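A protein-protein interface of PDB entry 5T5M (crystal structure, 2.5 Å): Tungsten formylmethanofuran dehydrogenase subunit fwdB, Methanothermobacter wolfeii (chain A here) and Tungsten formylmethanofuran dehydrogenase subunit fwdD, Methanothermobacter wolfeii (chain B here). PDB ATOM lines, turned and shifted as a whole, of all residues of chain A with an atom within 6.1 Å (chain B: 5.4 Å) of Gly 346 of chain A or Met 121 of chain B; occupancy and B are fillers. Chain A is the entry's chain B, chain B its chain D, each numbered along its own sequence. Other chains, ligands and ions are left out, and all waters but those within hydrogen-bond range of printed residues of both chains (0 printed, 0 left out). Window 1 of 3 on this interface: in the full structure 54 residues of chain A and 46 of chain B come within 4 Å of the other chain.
N of Pro 82 of chain B sits close to O of Ala 347 of chain A.
SD of Met 117 of chain B sits close to N of Pro 371 of chain A (3.7 Å).
The side-chain hydroxyl of Thr 372 of chain A sits at hydrogen-bond distance from the backbone NH of Gly 346 of chain A (2.8 Å).
The side-chain carboxylate of Asp 344 of chain A sits at hydrogen-bond distance from the backbone NH of Ala 347 of chain A (3.4 Å).
Met 121 of chain B touches Gly 346 of chain A.
Leu 354 of chain A touches Met 121 of chain B (CD1 to CE, 3.7 Å).
Leu 354 of chain A touches Tyr 124 of chain B.
Pro 371 of chain A touches Met 121 of chain B (CB to SD, 3.7 Å).
Met 117 of chain B touches Glu 374 of chain A (SD to CG, 3.98 Å).
OE1 of Glu 374 of chain A touches CB of Pro 118 of chain B, 3.6 Å away.
Met 121 of chain B touches Met 375 of chain A (CE to SD, 3.9 Å).
Met 375 of chain A touches Tyr 124 of chain B.
Asp 344 of chain A touches none of the printed residues of chain B.
Of the printed residues of chain B, Gly 346 of chain A touches Met 121 (3.7 Å).
Of the printed residues of chain B, Leu 354 of chain A touches Met 121 (3.7 Å) and Tyr 124 (3.5 Å).
Of the printed residues of chain B, Glu 374 of chain A touches Met 117 and Pro 118.
Printed residues of chain B within 4 Å of Met 375 of chain A: Met 121 (3.9 Å) and Tyr 124 (3.9 Å).
Of the printed residues of chain A, Pro 82 of chain B touches Ala 347.
Met 121 of chain B touches just these residues of chain A: Gly 346 (3.7 Å), Leu 354 (3.7 Å), Pro 371 (3.7 Å) and Met 375 (3.9 Å).
Lys 122 of chain B touches none of the printed residues of chain A.
The nearest printed residue of chain A that does not touch Pro 82 of chain B is Gly 346 of chain A (4.2 Å).
Hydrophobic or aromatic side chains of chain B that line the printed part of chain A: Pro 82, Met 117, Pro 118, Met 121 and Tyr 124.
Hydrophobic or aromatic side chains of chain A within 4 Å of the printed part of chain B: Ala 347, Leu 354, Pro 371 and Met 375.
Along chain A the printed residues that touch a printed residue of chain B span positions 346 to 375.
Among the printed residues, no Asp or Glu carboxylate lies within 4 Å of a Lys or Arg side-chain nitrogen of the other chain.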
ATOM      1  N   ASP A 344       7.619  18.563 -10.088  1.00  0.00           N
ATOM      2  CA  ASP A 344       6.169  18.714 -10.004  1.00  0.00           C
ATOM      3  C   ASP A 344       5.530  18.269 -11.314  1.00  0.00           C
ATOM      4  O   ASP A 344       5.037  19.092 -12.096  1.00  0.00           O
ATOM      5  CB  ASP A 344       5.802  20.157  -9.669  1.00  0.00           C
ATOM      6  CG  ASP A 344       4.330  20.321  -9.375  1.00  0.00           C
ATOM      7  OD1 ASP A 344       3.639  19.288  -9.225  1.00  0.00           O
ATOM      8  OD2 ASP A 344       3.867  21.479  -9.287  1.00  0.00           O
ATOM      9  N   PRO A 345       5.509  16.958 -11.580  1.00  0.00           N
ATOM     10  CA  PRO A 345       4.809  16.454 -12.779  1.00  0.00           C
ATOM     11  C   PRO A 345       3.313  16.704 -12.764  1.00  0.00           C
ATOM     12  O   PRO A 345       2.699  16.726 -13.839  1.00  0.00           O
ATOM     13  CB  PRO A 345       5.117  14.950 -12.757  1.00  0.00           C
ATOM     14  CG  PRO A 345       5.390  14.652 -11.315  1.00  0.00           C
ATOM     15  CD  PRO A 345       6.086  15.869 -10.776  1.00  0.00           C
ATOM     16  N   GLY A 346       2.698  16.871 -11.586  1.00  0.00           N
ATOM     17  CA  GLY A 346       1.290  17.219 -11.552  1.00  0.00           C
ATOM     18  C   GLY A 346       0.996  18.527 -12.261  1.00  0.00           C
ATOM     19  O   GLY A 346      -0.011  18.658 -12.964  1.00  0.00           O
ATOM     20  N   ALA A 347       1.870  19.517 -12.088  1.00  0.00           N
ATOM     21  CA  ALA A 347       1.675  20.799 -12.746  1.00  0.00           C
ATOM     22  C   ALA A 347       2.145  20.767 -14.187  1.00  0.00           C
ATOM     23  O   ALA A 347       1.631  21.520 -15.022  1.00  0.00           O
ATOM     24  CB  ALA A 347       2.434  21.896 -11.995  1.00  0.00           C
ATOM     25  N   HIS A 348       3.098  19.896 -14.499  1.00  0.00           N
ATOM     26  CA  HIS A 348       3.911  20.062 -15.690  1.00  0.00           C
ATOM     27  C   HIS A 348       3.977  18.821 -16.580  1.00  0.00           C
ATOM     28  O   HIS A 348       4.789  18.787 -17.511  1.00  0.00           O
ATOM     29  CB  HIS A 348       5.308  20.504 -15.254  1.00  0.00           C
ATOM     30  CG  HIS A 348       5.325  21.838 -14.578  1.00  0.00           C
ATOM     31  ND1 HIS A 348       6.089  22.095 -13.460  1.00  0.00           N
ATOM     32  CD2 HIS A 348       4.672  22.992 -14.859  1.00  0.00           C
ATOM     33  CE1 HIS A 348       5.911  23.350 -13.085  1.00  0.00           C
ATOM     34  NE2 HIS A 348       5.055  23.917 -13.918  1.00  0.00           N
ATOM     35  N   PHE A 349       3.160  17.802 -16.329  1.00  0.00           N
ATOM     36  CA  PHE A 349       2.944  16.760 -17.325  1.00  0.00           C
ATOM     37  C   PHE A 349       1.604  16.970 -18.010  1.00  0.00           C
ATOM     38  O   PHE A 349       0.717  17.643 -17.475  1.00  0.00           O
ATOM     39  CB  PHE A 349       2.962  15.367 -16.685  1.00  0.00           C
ATOM     40  CG  PHE A 349       4.341  14.792 -16.456  1.00  0.00           C
ATOM     41  CD1 PHE A 349       5.491  15.548 -16.649  1.00  0.00           C
ATOM     42  CD2 PHE A 349       4.479  13.470 -16.047  1.00  0.00           C
ATOM     43  CE1 PHE A 349       6.751  14.996 -16.427  1.00  0.00           C
ATOM     44  CE2 PHE A 349       5.743  12.911 -15.826  1.00  0.00           C
ATOM     45  CZ  PHE A 349       6.873  13.675 -16.017  1.00  0.00           C
ATOM     46  N   LEU A 354      -1.245  12.656 -16.381  1.00  0.00           N
ATOM     47  CA  LEU A 354      -1.923  12.855 -15.106  1.00  0.00           C
ATOM     48  C   LEU A 354      -3.015  11.818 -14.896  1.00  0.00           C
ATOM     49  O   LEU A 354      -3.268  11.412 -13.754  1.00  0.00           O
ATOM     50  CB  LEU A 354      -2.508  14.269 -15.033  1.00  0.00           C
ATOM     51  CG  LEU A 354      -1.664  15.371 -14.363  1.00  0.00           C
ATOM     52  CD1 LEU A 354      -1.570  15.137 -12.863  1.00  0.00           C
ATOM     53  CD2 LEU A 354      -0.281  15.475 -14.951  1.00  0.00           C
ATOM     54  N   MET A 357      -1.240   8.898 -13.209  1.00  0.00           N
ATOM     55  CA  MET A 357      -0.808   9.169 -11.842  1.00  0.00           C
ATOM     56  C   MET A 357      -1.968   9.074 -10.858  1.00  0.00           C
ATOM     57  O   MET A 357      -1.759   8.775  -9.675  1.00  0.00           O
ATOM     58  CB  MET A 357      -0.173  10.556 -11.753  1.00  0.00           C
ATOM     59  CG  MET A 357       1.123  10.713 -12.524  1.00  0.00           C
ATOM     60  SD  MET A 357       1.624  12.447 -12.675  1.00  0.00           S
ATOM     61  CE  MET A 357       1.946  12.867 -10.951  1.00  0.00           C
ATOM     62  N   PRO A 371       0.533  20.809  -7.182  1.00  0.00           N
ATOM     63  CA  PRO A 371      -0.367  19.832  -7.820  1.00  0.00           C
ATOM     64  C   PRO A 371       0.078  18.390  -7.662  1.00  0.00           C
ATOM     65  O   PRO A 371      -0.771  17.495  -7.609  1.00  0.00           O
ATOM     66  CB  PRO A 371      -0.345  20.267  -9.290  1.00  0.00           C
ATOM     67  CG  PRO A 371      -0.131  21.735  -9.232  1.00  0.00           C
ATOM     68  CD  PRO A 371       0.763  21.987  -8.038  1.00  0.00           C
ATOM     69  N   THR A 372       1.382  18.128  -7.597  1.00  0.00           N
ATOM     70  CA  THR A 372       1.844  16.764  -7.373  1.00  0.00           C
ATOM     71  C   THR A 372       1.442  16.278  -5.984  1.00  0.00           C
ATOM     72  O   THR A 372       0.933  15.160  -5.831  1.00  0.00           O
ATOM     73  CB  THR A 372       3.360  16.685  -7.566  1.00  0.00           C
ATOM     74  OG1 THR A 372       3.689  16.892  -8.954  1.00  0.00           O
ATOM     75  CG2 THR A 372       3.903  15.329  -7.124  1.00  0.00           C
ATOM     76  N   GLU A 374      -1.031  17.081  -4.392  1.00  0.00           N
ATOM     77  CA  GLU A 374      -2.464  16.803  -4.435  1.00  0.00           C
ATOM     78  C   GLU A 374      -2.748  15.398  -4.953  1.00  0.00           C
ATOM     79  O   GLU A 374      -3.714  14.761  -4.523  1.00  0.00           O
ATOM     80  CB  GLU A 374      -3.180  17.829  -5.316  1.00  0.00           C
ATOM     81  CG  GLU A 374      -3.104  19.261  -4.825  1.00  0.00           C
ATOM     82  CD  GLU A 374      -4.111  19.566  -3.737  1.00  0.00           C
ATOM     83  OE1 GLU A 374      -5.299  19.180  -3.884  1.00  0.00           O
ATOM     84  OE2 GLU A 374      -3.710  20.192  -2.733  1.00  0.00           O
ATOM     85  N   MET A 375      -1.935  14.908  -5.883  1.00  0.00           N
ATOM     86  CA  MET A 375      -2.090  13.569  -6.428  1.00  0.00           C
ATOM     87  C   MET A 375      -1.355  12.525  -5.606  1.00  0.00           C
ATOM     88  O   MET A 375      -1.297  11.362  -6.020  1.00  0.00           O
ATOM     89  CB  MET A 375      -1.569  13.507  -7.871  1.00  0.00           C
ATOM     90  CG  MET A 375      -2.005  14.638  -8.795  1.00  0.00           C
ATOM     91  SD  MET A 375      -3.738  14.587  -9.293  1.00  0.00           S
ATOM     92  CE  MET A 375      -3.849  12.978 -10.070  1.00  0.00           C
ATOM     93  N   PRO B  82      -0.620  23.560 -14.770  1.00  0.00           N
ATOM     94  CA  PRO B  82      -1.666  22.540 -14.927  1.00  0.00           C
ATOM     95  C   PRO B  82      -2.819  22.979 -15.809  1.00  0.00           C
ATOM     96  O   PRO B  82      -3.463  22.123 -16.428  1.00  0.00           O
ATOM     97  CB  PRO B  82      -2.115  22.292 -13.482  1.00  0.00           C
ATOM     98  CG  PRO B  82      -1.774  23.559 -12.757  1.00  0.00           C
ATOM     99  CD  PRO B  82      -0.488  24.004 -13.375  1.00  0.00           C
ATOM    100  N   ASP B 116      -9.205  27.082  -9.179  1.00  0.00           N
ATOM    101  CA  ASP B 116      -7.955  27.272  -8.460  1.00  0.00           C
ATOM    102  C   ASP B 116      -7.149  25.972  -8.511  1.00  0.00           C
ATOM    103  O   ASP B 116      -7.521  25.008  -9.186  1.00  0.00           O
ATOM    104  CB  ASP B 116      -8.218  27.752  -7.033  1.00  0.00           C
ATOM    105  CG  ASP B 116      -9.048  26.779  -6.218  1.00  0.00           C
ATOM    106  OD1 ASP B 116      -8.980  25.558  -6.470  1.00  0.00           O
ATOM    107  OD2 ASP B 116      -9.760  27.239  -5.303  1.00  0.00           O
ATOM    108  N   MET B 117      -6.022  25.931  -7.790  1.00  0.00           N
ATOM    109  CA  MET B 117      -5.083  24.825  -7.983  1.00  0.00           C
ATOM    110  C   MET B 117      -5.643  23.512  -7.451  1.00  0.00           C
ATOM    111  O   MET B 117      -5.725  22.539  -8.219  1.00  0.00           O
ATOM    112  CB  MET B 117      -3.726  25.181  -7.368  1.00  0.00           C
ATOM    113  CG  MET B 117      -2.617  24.220  -7.728  1.00  0.00           C
ATOM    114  SD  MET B 117      -2.640  22.741  -6.705  1.00  0.00           S
ATOM    115  CE  MET B 117      -1.839  23.355  -5.220  1.00  0.00           C
ATOM    116  N   PRO B 118      -6.056  23.404  -6.184  1.00  0.00           N
ATOM    117  CA  PRO B 118      -6.561  22.103  -5.700  1.00  0.00           C
ATOM    118  C   PRO B 118      -7.788  21.623  -6.452  1.00  0.00           C
ATOM    119  O   PRO B 118      -7.967  20.410  -6.631  1.00  0.00           O
ATOM    120  CB  PRO B 118      -6.883  22.373  -4.223  1.00  0.00           C
ATOM    121  CG  PRO B 118      -6.237  23.679  -3.892  1.00  0.00           C
ATOM    122  CD  PRO B 118      -6.198  24.456  -5.162  1.00  0.00           C
ATOM    123  N   THR B 119      -8.638  22.555  -6.893  1.00  0.00           N
ATOM    124  CA  THR B 119      -9.880  22.207  -7.573  1.00  0.00           C
ATOM    125  C   THR B 119      -9.619  21.716  -8.989  1.00  0.00           C
ATOM    126  O   THR B 119     -10.276  20.778  -9.458  1.00  0.00           O
ATOM    127  CB  THR B 119     -10.799  23.423  -7.612  1.00  0.00           C
ATOM    128  OG1 THR B 119     -11.010  23.901  -6.280  1.00  0.00           O
ATOM    129  CG2 THR B 119     -12.130  23.077  -8.258  1.00  0.00           C
ATOM    130  N   LEU B 120      -8.695  22.361  -9.700  1.00  0.00           N
ATOM    131  CA  LEU B 120      -8.410  21.942 -11.063  1.00  0.00           C
ATOM    132  C   LEU B 120      -7.918  20.504 -11.088  1.00  0.00           C
ATOM    133  O   LEU B 120      -8.300  19.724 -11.969  1.00  0.00           O
ATOM    134  CB  LEU B 120      -7.381  22.878 -11.695  1.00  0.00           C
ATOM    135  CG  LEU B 120      -7.019  22.610 -13.165  1.00  0.00           C
ATOM    136  CD1 LEU B 120      -8.075  23.146 -14.117  1.00  0.00           C
ATOM    137  CD2 LEU B 120      -5.654  23.204 -13.491  1.00  0.00           C
ATOM    138  N   MET B 121      -7.084  20.127 -10.117  1.00  0.00           N
ATOM    139  CA  MET B 121      -6.528  18.780 -10.101  1.00  0.00           C
ATOM    140  C   MET B 121      -7.592  17.725  -9.839  1.00  0.00           C
ATOM    141  O   MET B 121      -7.343  16.542 -10.098  1.00  0.00           O
ATOM    142  CB  MET B 121      -5.428  18.683  -9.044  1.00  0.00           C
ATOM    143  CG  MET B 121      -4.283  19.684  -9.228  1.00  0.00           C
ATOM    144  SD  MET B 121      -3.616  19.674 -10.902  1.00  0.00           S
ATOM    145  CE  MET B 121      -3.060  17.974 -11.040  1.00  0.00           C
ATOM    146  N   LYS B 122      -8.767  18.123  -9.342  1.00  0.00           N
ATOM    147  CA  LYS B 122      -9.840  17.168  -9.081  1.00  0.00           C
ATOM    148  C   LYS B 122     -10.356  16.512 -10.354  1.00  0.00           C
ATOM    149  O   LYS B 122     -10.941  15.428 -10.280  1.00  0.00           O
ATOM    150  CB  LYS B 122     -11.008  17.849  -8.369  1.00  0.00           C
ATOM    151  CG  LYS B 122     -10.654  18.450  -7.020  1.00  0.00           C
ATOM    152  CD  LYS B 122     -10.304  17.389  -5.985  1.00  0.00           C
ATOM    153  CE  LYS B 122     -10.285  17.976  -4.570  1.00  0.00           C
ATOM    154  NZ  LYS B 122     -10.031  16.927  -3.545  1.00  0.00           N
ATOM    155  N   VAL B 123     -10.159  17.136 -11.514  1.00  0.00           N
ATOM    156  CA  VAL B 123     -10.658  16.567 -12.756  1.00  0.00           C
ATOM    157  C   VAL B 123     -10.019  15.223 -13.070  1.00  0.00           C
ATOM    158  O   VAL B 123     -10.536  14.489 -13.914  1.00  0.00           O
ATOM    159  CB  VAL B 123     -10.446  17.548 -13.939  1.00  0.00           C
ATOM    160  CG1 VAL B 123     -10.980  18.948 -13.596  1.00  0.00           C
ATOM    161  CG2 VAL B 123      -8.979  17.611 -14.360  1.00  0.00           C
ATOM    162  N   TYR B 124      -8.916  14.877 -12.407  1.00  0.00           N
ATOM    163  CA  TYR B 124      -8.220  13.623 -12.661  1.00  0.00           C
ATOM    164  C   TYR B 124      -8.655  12.499 -11.722  1.00  0.00           C
ATOM    165  O   TYR B 124      -8.027  11.436 -11.715  1.00  0.00           O
ATOM    166  CB  TYR B 124      -6.702  13.843 -12.575  1.00  0.00           C
ATOM    167  CG  TYR B 124      -6.196  14.786 -13.652  1.00  0.00           C
ATOM    168  CD1 TYR B 124      -6.141  14.391 -14.988  1.00  0.00           C
ATOM    169  CD2 TYR B 124      -5.803  16.076 -13.340  1.00  0.00           C
ATOM    170  CE1 TYR B 124      -5.701  15.253 -15.968  1.00  0.00           C
ATOM    171  CE2 TYR B 124      -5.359  16.942 -14.310  1.00  0.00           C
ATOM    172  CZ  TYR B 124      -5.308  16.533 -15.622  1.00  0.00           C
ATOM    173  OH  TYR B 124      -4.860  17.413 -16.588  1.00  0.00           O
ATOM    174  N   GLY B 125      -9.712  12.704 -10.941  1.00  0.00           N
ATOM    175  CA  GLY B 125     -10.364  11.622 -10.224  1.00  0.00           C
ATOM    176  C   GLY B 125      -9.448  10.750  -9.389  1.00  0.00           C
ATOM    177  O   GLY B 125      -9.535   9.517  -9.442  1.00  0.00           O
